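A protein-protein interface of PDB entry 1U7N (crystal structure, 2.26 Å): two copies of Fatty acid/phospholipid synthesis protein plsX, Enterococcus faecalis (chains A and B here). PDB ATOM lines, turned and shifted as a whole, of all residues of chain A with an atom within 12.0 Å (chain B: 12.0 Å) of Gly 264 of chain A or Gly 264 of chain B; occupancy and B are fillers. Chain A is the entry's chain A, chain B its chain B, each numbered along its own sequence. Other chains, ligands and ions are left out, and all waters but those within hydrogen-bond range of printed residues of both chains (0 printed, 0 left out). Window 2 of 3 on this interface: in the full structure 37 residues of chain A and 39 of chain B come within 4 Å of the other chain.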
ATOM      1  N   LEU A 250     -19.281  18.938  13.197  1.00  0.00           N
ATOM      2  CA  LEU A 250     -18.402  18.316  12.217  1.00  0.00           C
ATOM      3  C   LEU A 250     -17.775  17.016  12.724  1.00  0.00           C
ATOM      4  O   LEU A 250     -17.740  16.034  11.986  1.00  0.00           O
ATOM      5  CB  LEU A 250     -17.302  19.280  11.766  1.00  0.00           C
ATOM      6  CG  LEU A 250     -17.676  20.474  10.905  1.00  0.00           C
ATOM      7  CD1 LEU A 250     -16.419  21.162  10.502  1.00  0.00           C
ATOM      8  CD2 LEU A 250     -18.457  20.081   9.664  1.00  0.00           C
ATOM      9  N   LYS A 251     -17.277  17.020  13.965  1.00  0.00           N
ATOM     10  CA  LYS A 251     -16.653  15.834  14.572  1.00  0.00           C
ATOM     11  C   LYS A 251     -17.591  14.647  14.525  1.00  0.00           C
ATOM     12  O   LYS A 251     -17.176  13.550  14.174  1.00  0.00           O
ATOM     13  CB  LYS A 251     -16.266  16.071  16.035  1.00  0.00           C
ATOM     14  CG  LYS A 251     -15.002  16.862  16.277  1.00  0.00           C
ATOM     15  CD  LYS A 251     -14.978  17.432  17.713  1.00  0.00           C
ATOM     16  CE  LYS A 251     -13.806  18.385  17.945  1.00  0.00           C
ATOM     17  NZ  LYS A 251     -13.585  18.612  19.419  1.00  0.00           N
ATOM     18  N   THR A 252     -18.849  14.877  14.899  1.00  0.00           N
ATOM     19  CA  THR A 252     -19.890  13.842  14.949  1.00  0.00           C
ATOM     20  C   THR A 252     -20.201  13.252  13.565  1.00  0.00           C
ATOM     21  O   THR A 252     -20.445  12.056  13.447  1.00  0.00           O
ATOM     22  CB  THR A 252     -21.173  14.401  15.625  1.00  0.00           C
ATOM     23  OG1 THR A 252     -20.901  14.615  17.009  1.00  0.00           O
ATOM     24  CG2 THR A 252     -22.351  13.443  15.516  1.00  0.00           C
ATOM     25  N   ALA A 253     -20.203  14.104  12.536  1.00  0.00           N
ATOM     26  CA  ALA A 253     -20.371  13.669  11.152  1.00  0.00           C
ATOM     27  C   ALA A 253     -19.128  12.911  10.655  1.00  0.00           C
ATOM     28  O   ALA A 253     -19.247  11.955   9.891  1.00  0.00           O
ATOM     29  CB  ALA A 253     -20.677  14.850  10.248  1.00  0.00           C
ATOM     30  N   ILE A 254     -17.949  13.347  11.093  1.00  0.00           N
ATOM     31  CA  ILE A 254     -16.692  12.676  10.785  1.00  0.00           C
ATOM     32  C   ILE A 254     -16.656  11.292  11.438  1.00  0.00           C
ATOM     33  O   ILE A 254     -16.256  10.313  10.800  1.00  0.00           O
ATOM     34  CB  ILE A 254     -15.465  13.542  11.206  1.00  0.00           C
ATOM     35  CG1 ILE A 254     -15.275  14.708  10.233  1.00  0.00           C
ATOM     36  CG2 ILE A 254     -14.181  12.711  11.284  1.00  0.00           C
ATOM     37  CD1 ILE A 254     -14.514  15.881  10.821  1.00  0.00           C
ATOM     38  N   LEU A 255     -17.105  11.213  12.690  1.00  0.00           N
ATOM     39  CA  LEU A 255     -17.142   9.955  13.448  1.00  0.00           C
ATOM     40  C   LEU A 255     -18.276   9.017  13.026  1.00  0.00           C
ATOM     41  O   LEU A 255     -18.377   7.898  13.533  1.00  0.00           O
ATOM     42  CB  LEU A 255     -17.198  10.215  14.965  1.00  0.00           C
ATOM     43  CG  LEU A 255     -15.966  10.843  15.634  1.00  0.00           C
ATOM     44  CD1 LEU A 255     -16.197  11.110  17.127  1.00  0.00           C
ATOM     45  CD2 LEU A 255     -14.708  10.001  15.424  1.00  0.00           C
ATOM     46  N   SER A 256     -19.122   9.472  12.102  1.00  0.00           N
ATOM     47  CA  SER A 256     -20.187   8.635  11.552  1.00  0.00           C
ATOM     48  C   SER A 256     -19.664   7.648  10.508  1.00  0.00           C
ATOM     49  O   SER A 256     -20.435   6.872   9.934  1.00  0.00           O
ATOM     50  CB  SER A 256     -21.297   9.501  10.961  1.00  0.00           C
ATOM     51  OG  SER A 256     -22.147   9.966  11.993  1.00  0.00           O
ATOM     52  N   GLY A 264     -14.488  10.987   0.778  1.00  0.00           N
ATOM     53  CA  GLY A 264     -15.612  11.880   1.096  1.00  0.00           C
ATOM     54  C   GLY A 264     -15.555  12.434   2.515  1.00  0.00           C
ATOM     55  O   GLY A 264     -15.905  13.609   2.756  1.00  0.00           O
ATOM     56  N   ALA A 265     -15.133  11.585   3.457  1.00  0.00           N
ATOM     57  CA  ALA A 265     -14.919  11.985   4.845  1.00  0.00           C
ATOM     58  C   ALA A 265     -13.703  12.916   4.975  1.00  0.00           C
ATOM     59  O   ALA A 265     -13.535  13.607   5.976  1.00  0.00           O
ATOM     60  CB  ALA A 265     -14.743  10.754   5.730  1.00  0.00           C
ATOM     61  N   LEU A 266     -12.868  12.937   3.949  1.00  0.00           N
ATOM     62  CA  LEU A 266     -11.635  13.702   3.978  1.00  0.00           C
ATOM     63  C   LEU A 266     -11.846  15.207   3.843  1.00  0.00           C
ATOM     64  O   LEU A 266     -11.100  15.984   4.433  1.00  0.00           O
ATOM     65  CB  LEU A 266     -10.693  13.220   2.876  1.00  0.00           C
ATOM     66  CG  LEU A 266      -9.195  13.312   3.146  1.00  0.00           C
ATOM     67  CD1 LEU A 266      -8.845  12.919   4.582  1.00  0.00           C
ATOM     68  CD2 LEU A 266      -8.463  12.433   2.149  1.00  0.00           C
ATOM     69  N   LEU A 267     -12.836  15.603   3.043  1.00  0.00           N
ATOM     70  CA  LEU A 267     -13.200  17.006   2.893  1.00  0.00           C
ATOM     71  C   LEU A 267     -13.719  17.581   4.224  1.00  0.00           C
ATOM     72  O   LEU A 267     -13.470  18.734   4.555  1.00  0.00           O
ATOM     73  CB  LEU A 267     -14.242  17.174   1.792  1.00  0.00           C
ATOM     74  CG  LEU A 267     -13.786  16.833   0.371  1.00  0.00           C
ATOM     75  CD1 LEU A 267     -14.100  15.377   0.045  1.00  0.00           C
ATOM     76  CD2 LEU A 267     -14.447  17.765  -0.648  1.00  0.00           C
ATOM     77  N   LEU A 268     -14.407  16.731   4.972  1.00  0.00           N
ATOM     78  CA  LEU A 268     -14.998  17.051   6.252  1.00  0.00           C
ATOM     79  C   LEU A 268     -13.941  17.155   7.369  1.00  0.00           C
ATOM     80  O   LEU A 268     -14.051  18.011   8.247  1.00  0.00           O
ATOM     81  CB  LEU A 268     -16.034  15.969   6.579  1.00  0.00           C
ATOM     82  CG  LEU A 268     -17.359  16.267   7.285  1.00  0.00           C
ATOM     83  CD1 LEU A 268     -18.042  17.555   6.789  1.00  0.00           C
ATOM     84  CD2 LEU A 268     -18.286  15.061   7.141  1.00  0.00           C
ATOM     85  N   LYS A 269     -12.932  16.278   7.335  1.00  0.00           N
ATOM     86  CA  LYS A 269     -11.821  16.335   8.279  1.00  0.00           C
ATOM     87  C   LYS A 269     -10.957  17.551   8.012  1.00  0.00           C
ATOM     88  O   LYS A 269     -10.473  18.176   8.955  1.00  0.00           O
ATOM     89  CB  LYS A 269     -10.960  15.079   8.234  1.00  0.00           C
ATOM     90  CG  LYS A 269     -11.592  13.848   8.847  1.00  0.00           C
ATOM     91  CD  LYS A 269     -10.535  12.789   9.150  1.00  0.00           C
ATOM     92  CE  LYS A 269      -9.939  12.965  10.550  1.00  0.00           C
ATOM     93  NZ  LYS A 269     -10.705  12.257  11.646  1.00  0.00           N
ATOM     94  N   ASN A 270     -10.770  17.870   6.733  1.00  0.00           N
ATOM     95  CA  ASN A 270     -10.079  19.079   6.303  1.00  0.00           C
ATOM     96  C   ASN A 270     -10.818  20.377   6.697  1.00  0.00           C
ATOM     97  O   ASN A 270     -10.188  21.397   6.996  1.00  0.00           O
ATOM     98  CB  ASN A 270      -9.870  19.065   4.787  1.00  0.00           C
ATOM     99  CG  ASN A 270      -8.892  17.976   4.316  1.00  0.00           C
ATOM    100  OD1 ASN A 270      -8.332  17.220   5.116  1.00  0.00           O
ATOM    101  ND2 ASN A 270      -8.702  17.894   2.985  1.00  0.00           N
ATOM    102  N   ALA A 271     -12.147  20.335   6.644  1.00  0.00           N
ATOM    103  CA  ALA A 271     -12.986  21.461   7.049  1.00  0.00           C
ATOM    104  C   ALA A 271     -12.844  21.722   8.543  1.00  0.00           C
ATOM    105  O   ALA A 271     -12.720  22.865   8.942  1.00  0.00           O
ATOM    106  CB  ALA A 271     -14.458  21.212   6.683  1.00  0.00           C
ATOM    107  N   LEU A 272     -12.872  20.652   9.336  1.00  0.00           N
ATOM    108  CA  LEU A 272     -12.711  20.711  10.766  1.00  0.00           C
ATOM    109  C   LEU A 272     -11.339  21.227  11.180  1.00  0.00           C
ATOM    110  O   LEU A 272     -11.241  22.071  12.092  1.00  0.00           O
ATOM    111  CB  LEU A 272     -12.973  19.350  11.424  1.00  0.00           C
ATOM    112  CG  LEU A 272     -12.750  19.359  12.945  1.00  0.00           C
ATOM    113  CD1 LEU A 272     -13.814  20.214  13.652  1.00  0.00           C
ATOM    114  CD2 LEU A 272     -12.684  17.987  13.565  1.00  0.00           C
ATOM    115  N   HIS A 273     -10.300  20.719  10.504  1.00  0.00           N
ATOM    116  CA  HIS A 273      -8.908  21.129  10.718  1.00  0.00           C
ATOM    117  C   HIS A 273      -8.730  22.618  10.411  1.00  0.00           C
ATOM    118  O   HIS A 273      -8.136  23.333  11.203  1.00  0.00           O
ATOM    119  CB  HIS A 273      -7.944  20.239   9.892  1.00  0.00           C
ATOM    120  CG  HIS A 273      -6.560  20.802   9.720  1.00  0.00           C
ATOM    121  ND1 HIS A 273      -5.586  20.723  10.699  1.00  0.00           N
ATOM    122  CD2 HIS A 273      -5.977  21.431   8.667  1.00  0.00           C
ATOM    123  CE1 HIS A 273      -4.475  21.297  10.264  1.00  0.00           C
ATOM    124  NE2 HIS A 273      -4.685  21.733   9.034  1.00  0.00           N
ATOM    125  N   LEU B 249     -16.886  29.327   6.229  1.00  0.00           N
ATOM    126  CA  LEU B 249     -15.729  28.473   5.971  1.00  0.00           C
ATOM    127  C   LEU B 249     -16.148  27.230   5.187  1.00  0.00           C
ATOM    128  O   LEU B 249     -15.461  26.841   4.263  1.00  0.00           O
ATOM    129  CB  LEU B 249     -14.975  28.096   7.256  1.00  0.00           C
ATOM    130  CG  LEU B 249     -14.366  29.192   8.155  1.00  0.00           C
ATOM    131  CD1 LEU B 249     -13.697  28.578   9.394  1.00  0.00           C
ATOM    132  CD2 LEU B 249     -13.394  30.097   7.399  1.00  0.00           C
ATOM    133  N   LEU B 250     -17.285  26.633   5.554  1.00  0.00           N
ATOM    134  CA  LEU B 250     -17.833  25.523   4.809  1.00  0.00           C
ATOM    135  C   LEU B 250     -18.262  25.949   3.411  1.00  0.00           C
ATOM    136  O   LEU B 250     -17.874  25.303   2.450  1.00  0.00           O
ATOM    137  CB  LEU B 250     -18.985  24.843   5.546  1.00  0.00           C
ATOM    138  CG  LEU B 250     -18.759  24.122   6.875  1.00  0.00           C
ATOM    139  CD1 LEU B 250     -19.778  23.006   6.983  1.00  0.00           C
ATOM    140  CD2 LEU B 250     -17.353  23.555   7.034  1.00  0.00           C
ATOM    141  N   LYS B 251     -19.029  27.038   3.305  1.00  0.00           N
ATOM    142  CA  LYS B 251     -19.473  27.583   2.006  1.00  0.00           C
ATOM    143  C   LYS B 251     -18.356  27.814   1.001  1.00  0.00           C
ATOM    144  O   LYS B 251     -18.543  27.563  -0.192  1.00  0.00           O
ATOM    145  CB  LYS B 251     -20.216  28.894   2.158  1.00  0.00           C
ATOM    146  CG  LYS B 251     -21.594  28.791   2.740  1.00  0.00           C
ATOM    147  CD  LYS B 251     -22.198  30.195   2.822  1.00  0.00           C
ATOM    148  CE  LYS B 251     -23.029  30.385   4.078  1.00  0.00           C
ATOM    149  NZ  LYS B 251     -23.937  31.552   3.920  1.00  0.00           N
ATOM    150  N   THR B 252     -17.221  28.323   1.481  1.00  0.00           N
ATOM    151  CA  THR B 252     -16.024  28.471   0.648  1.00  0.00           C
ATOM    152  C   THR B 252     -15.413  27.118   0.220  1.00  0.00           C
ATOM    153  O   THR B 252     -14.928  27.003  -0.908  1.00  0.00           O
ATOM    154  CB  THR B 252     -14.957  29.376   1.313  1.00  0.00           C
ATOM    155  OG1 THR B 252     -15.514  30.675   1.569  1.00  0.00           O
ATOM    156  CG2 THR B 252     -13.744  29.532   0.410  1.00  0.00           C
ATOM    157  N   ALA B 253     -15.447  26.108   1.100  1.00  0.00           N
ATOM    158  CA  ALA B 253     -14.952  24.767   0.749  1.00  0.00           C
ATOM    159  C   ALA B 253     -15.826  24.143  -0.345  1.00  0.00           C
ATOM    160  O   ALA B 253     -15.339  23.845  -1.433  1.00  0.00           O
ATOM    161  CB  ALA B 253     -14.865  23.866   1.967  1.00  0.00           C
ATOM    162  N   ILE B 254     -17.113  23.954  -0.052  1.00  0.00           N
ATOM    163  CA  ILE B 254     -18.127  23.814  -1.094  1.00  0.00           C
ATOM    164  C   ILE B 254     -17.862  25.014  -1.996  1.00  0.00           C
ATOM    165  O   ILE B 254     -17.349  26.023  -1.520  1.00  0.00           O
ATOM    166  CB  ILE B 254     -19.549  23.944  -0.495  1.00  0.00           C
ATOM    167  CG1 ILE B 254     -19.725  23.025   0.715  1.00  0.00           C
ATOM    168  CG2 ILE B 254     -20.610  23.657  -1.543  1.00  0.00           C
ATOM    169  CD1 ILE B 254     -20.770  23.487   1.702  1.00  0.00           C
ATOM    170  N   LEU B 255     -18.156  24.935  -3.285  1.00  0.00           N
ATOM    171  CA  LEU B 255     -17.903  26.094  -4.169  1.00  0.00           C
ATOM    172  C   LEU B 255     -16.432  26.240  -4.581  1.00  0.00           C
ATOM    173  O   LEU B 255     -16.096  27.084  -5.417  1.00  0.00           O
ATOM    174  CB  LEU B 255     -18.438  27.404  -3.552  1.00  0.00           C
ATOM    175  CG  LEU B 255     -19.897  27.764  -3.877  1.00  0.00           C
ATOM    176  CD1 LEU B 255     -20.714  28.119  -2.637  1.00  0.00           C
ATOM    177  CD2 LEU B 255     -19.952  28.892  -4.909  1.00  0.00           C
ATOM    178  N   SER B 256     -15.562  25.422  -3.991  1.00  0.00           N
ATOM    179  CA  SER B 256     -14.199  25.270  -4.487  1.00  0.00           C
ATOM    180  C   SER B 256     -14.059  23.963  -5.259  1.00  0.00           C
ATOM    181  O   SER B 256     -13.437  23.935  -6.320  1.00  0.00           O
ATOM    182  CB  SER B 256     -13.180  25.333  -3.353  1.00  0.00           C
ATOM    183  OG  SER B 256     -12.630  26.632  -3.264  1.00  0.00           O
ATOM    184  N   GLY B 264     -17.818  13.892  -2.468  1.00  0.00           N
ATOM    185  CA  GLY B 264     -17.451  14.305  -1.117  1.00  0.00           C
ATOM    186  C   GLY B 264     -17.798  15.755  -0.842  1.00  0.00           C
ATOM    187  O   GLY B 264     -17.615  16.246   0.280  1.00  0.00           O
ATOM    188  N   ALA B 265     -18.285  16.442  -1.879  1.00  0.00           N
ATOM    189  CA  ALA B 265     -18.791  17.804  -1.769  1.00  0.00           C
ATOM    190  C   ALA B 265     -20.146  17.787  -1.053  1.00  0.00           C
ATOM    191  O   ALA B 265     -20.543  18.755  -0.392  1.00  0.00           O
ATOM    192  CB  ALA B 265     -18.929  18.411  -3.148  1.00  0.00           C
ATOM    193  N   LEU B 266     -20.826  16.650  -1.179  1.00  0.00           N
ATOM    194  CA  LEU B 266     -22.141  16.423  -0.623  1.00  0.00           C
ATOM    195  C   LEU B 266     -22.122  16.314   0.896  1.00  0.00           C
ATOM    196  O   LEU B 266     -23.059  16.753   1.581  1.00  0.00           O
ATOM    197  CB  LEU B 266     -22.723  15.143  -1.223  1.00  0.00           C
ATOM    198  CG  LEU B 266     -24.219  15.086  -1.489  1.00  0.00           C
ATOM    199  CD1 LEU B 266     -24.656  16.331  -2.231  1.00  0.00           C
ATOM    200  CD2 LEU B 266     -24.543  13.835  -2.306  1.00  0.00           C
ATOM    201  N   LEU B 267     -21.065  15.717   1.424  1.00  0.00           N
ATOM    202  CA  LEU B 267     -20.939  15.579   2.857  1.00  0.00           C
ATOM    203  C   LEU B 267     -20.724  16.952   3.492  1.00  0.00           C
ATOM    204  O   LEU B 267     -21.144  17.175   4.616  1.00  0.00           O
ATOM    205  CB  LEU B 267     -19.816  14.615   3.211  1.00  0.00           C
ATOM    206  CG  LEU B 267     -20.138  13.122   3.152  1.00  0.00           C
ATOM    207  CD1 LEU B 267     -18.976  12.358   2.539  1.00  0.00           C
ATOM    208  CD2 LEU B 267     -20.438  12.591   4.539  1.00  0.00           C
ATOM    209  N   LEU B 268     -20.101  17.867   2.751  1.00  0.00           N
ATOM    210  CA  LEU B 268     -19.925  19.253   3.188  1.00  0.00           C
ATOM    211  C   LEU B 268     -21.236  20.051   3.202  1.00  0.00           C
ATOM    212  O   LEU B 268     -21.576  20.669   4.216  1.00  0.00           O
ATOM    213  CB  LEU B 268     -18.865  19.979   2.336  1.00  0.00           C
ATOM    214  CG  LEU B 268     -17.377  19.775   2.652  1.00  0.00           C
ATOM    215  CD1 LEU B 268     -16.524  20.460   1.586  1.00  0.00           C
ATOM    216  CD2 LEU B 268     -17.019  20.293   4.050  1.00  0.00           C
ATOM    217  N   LYS B 269     -21.978  20.028   2.099  1.00  0.00           N
ATOM    218  CA  LYS B 269     -23.240  20.762   2.041  1.00  0.00           C
ATOM    219  C   LYS B 269     -24.273  20.239   3.037  1.00  0.00           C
ATOM    220  O   LYS B 269     -25.081  21.008   3.536  1.00  0.00           O
ATOM    221  CB  LYS B 269     -23.795  20.874   0.609  1.00  0.00           C
ATOM    222  CG  LYS B 269     -23.849  19.587  -0.210  1.00  0.00           C
ATOM    223  CD  LYS B 269     -23.389  19.827  -1.660  1.00  0.00           C
ATOM    224  CE  LYS B 269     -24.261  20.820  -2.404  1.00  0.00           C
ATOM    225  NZ  LYS B 269     -23.459  21.635  -3.371  1.00  0.00           N
ATOM    226  N   ASN B 270     -24.228  18.943   3.339  1.00  0.00           N
ATOM    227  CA  ASN B 270     -25.046  18.381   4.407  1.00  0.00           C
ATOM    228  C   ASN B 270     -24.606  18.906   5.784  1.00  0.00           C
ATOM    229  O   ASN B 270     -25.427  19.080   6.688  1.00  0.00           O
ATOM    230  CB  ASN B 270     -24.974  16.852   4.406  1.00  0.00           C
ATOM    231  CG  ASN B 270     -25.701  16.204   3.212  1.00  0.00           C
ATOM    232  OD1 ASN B 270     -26.373  16.873   2.419  1.00  0.00           O
ATOM    233  ND2 ASN B 270     -25.555  14.885   3.093  1.00  0.00           N
ATOM    234  N   ALA B 271     -23.298  19.127   5.935  1.00  0.00           N
ATOM    235  CA  ALA B 271     -22.737  19.632   7.187  1.00  0.00           C
ATOM    236  C   ALA B 271     -23.157  21.097   7.356  1.00  0.00           C
ATOM    237  O   ALA B 271     -23.651  21.477   8.396  1.00  0.00           O
ATOM    238  CB  ALA B 271     -21.199  19.469   7.216  1.00  0.00           C
ATOM    239  N   LEU B 272     -23.000  21.890   6.304  1.00  0.00           N
ATOM    240  CA  LEU B 272     -23.461  23.267   6.312  1.00  0.00           C
ATOM    241  C   LEU B 272     -24.965  23.375   6.593  1.00  0.00           C
ATOM    242  O   LEU B 272     -25.384  24.154   7.452  1.00  0.00           O
ATOM    243  CB  LEU B 272     -23.085  23.964   5.002  1.00  0.00           C
ATOM    244  CG  LEU B 272     -23.606  25.380   4.750  1.00  0.00           C
ATOM    245  CD1 LEU B 272     -23.091  26.395   5.783  1.00  0.00           C
ATOM    246  CD2 LEU B 272     -23.260  25.826   3.356  1.00  0.00           C
ATOM    247  N   HIS B 273     -25.766  22.588   5.879  1.00  0.00           N
ATOM    248  CA  HIS B 273     -27.215  22.585   6.053  1.00  0.00           C
ATOM    249  C   HIS B 273     -27.605  22.232   7.473  1.00  0.00           C
ATOM    250  O   HIS B 273     -28.475  22.876   8.034  1.00  0.00           O
ATOM    251  CB  HIS B 273     -27.882  21.625   5.060  1.00  0.00           C
ATOM    252  CG  HIS B 273     -29.352  21.433   5.286  1.00  0.00           C
ATOM    253  ND1 HIS B 273     -30.309  22.237   4.700  1.00  0.00           N
ATOM    254  CD2 HIS B 273     -30.028  20.519   6.026  1.00  0.00           C
ATOM    255  CE1 HIS B 273     -31.510  21.831   5.080  1.00  0.00           C
ATOM    256  NE2 HIS B 273     -31.367  20.796   5.891  1.00  0.00           N
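Of chain B, only Gly 264 (3.8 Å) and Leu 267 (3.3 Å) come within 4 Å of Gly 264 of chain A.
No residue of chain B comes within 4 Å of Ala 265 of chain A.
No residue of chain B comes within 4 Å of Leu 266 of chain A.
Leu 267 of chain A touches just these residues of chain B: Gly 264 (3.6 Å) and Leu 268 (3.9 Å).
Of the printed residues of chain A, Leu 250 of chain B touches Ala 271.
Gly 264 of chain B touches two residues of chain A.
Printed residues of chain A within 4 Å of Leu 268 of chain B: Leu 267 and Ala 271.
The nearest residue of chain B that does not touch Gly 264 of chain A is Ala 265 of chain B (5.9 Å).
The nearest printed residue of chain A that does not touch Ala 271 of chain B is Ala 253 of chain A (5.5 Å).
Hydrophobic or aromatic side chains of chain B that line the printed part of chain A: Leu 250, Leu 267, Leu 268 and Ala 271.
Of the 17 printed residues of chain A, 5 touch a printed residue of chain B.
Among the printed residues, no Asp or Glu carboxylate lies within 4 Å of a Lys or Arg side-chain nitrogen of the other chain.
Among the printed residues, merely in contact across the chains: Leu 250 of chain A with Ala 271 of chain B, Gly 264 of chain A with Gly 264 of chain B, Gly 264 of chain A with Leu 267 of chain B, Leu 267 of chain A with Gly 264 of chain B, Leu 267 of chain A with Leu 268 of chain B, Leu 268 of chain A with Leu 267 of chain B, Leu 268 of chain A with Ala 271 of chain B, Ala 271 of chain A with Leu 250 of chain B and Ala 271 of chain A with Leu 268 of chain B.
Leu 250 of chain A touches Ala 271 of chain B, and with the chains exchanged Ala 271 of chain A touches Leu 250 of chain B.
Gly 264 of chain B touches its own counterpart, Gly 264 of chain A.
Leu 267 of chain A touches Leu 268 of chain B, and with the chains exchanged Leu 268 of chain A touches Leu 267 of chain B.
Leu 268 of chain A touches Ala 271 of chain B, and with the chains exchanged Ala 271 of chain A touches Leu 268 of chain B.
Positions printed for both chains: 250, 251, 252, 253, 254, 255, 256, 264, 265, 266, 267, 268, 269, 270, 271, 272 and 273.
Of the 9 pairs that touch across the chains among the printed residues, 9 have their exchanged pair printed and touching as well.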
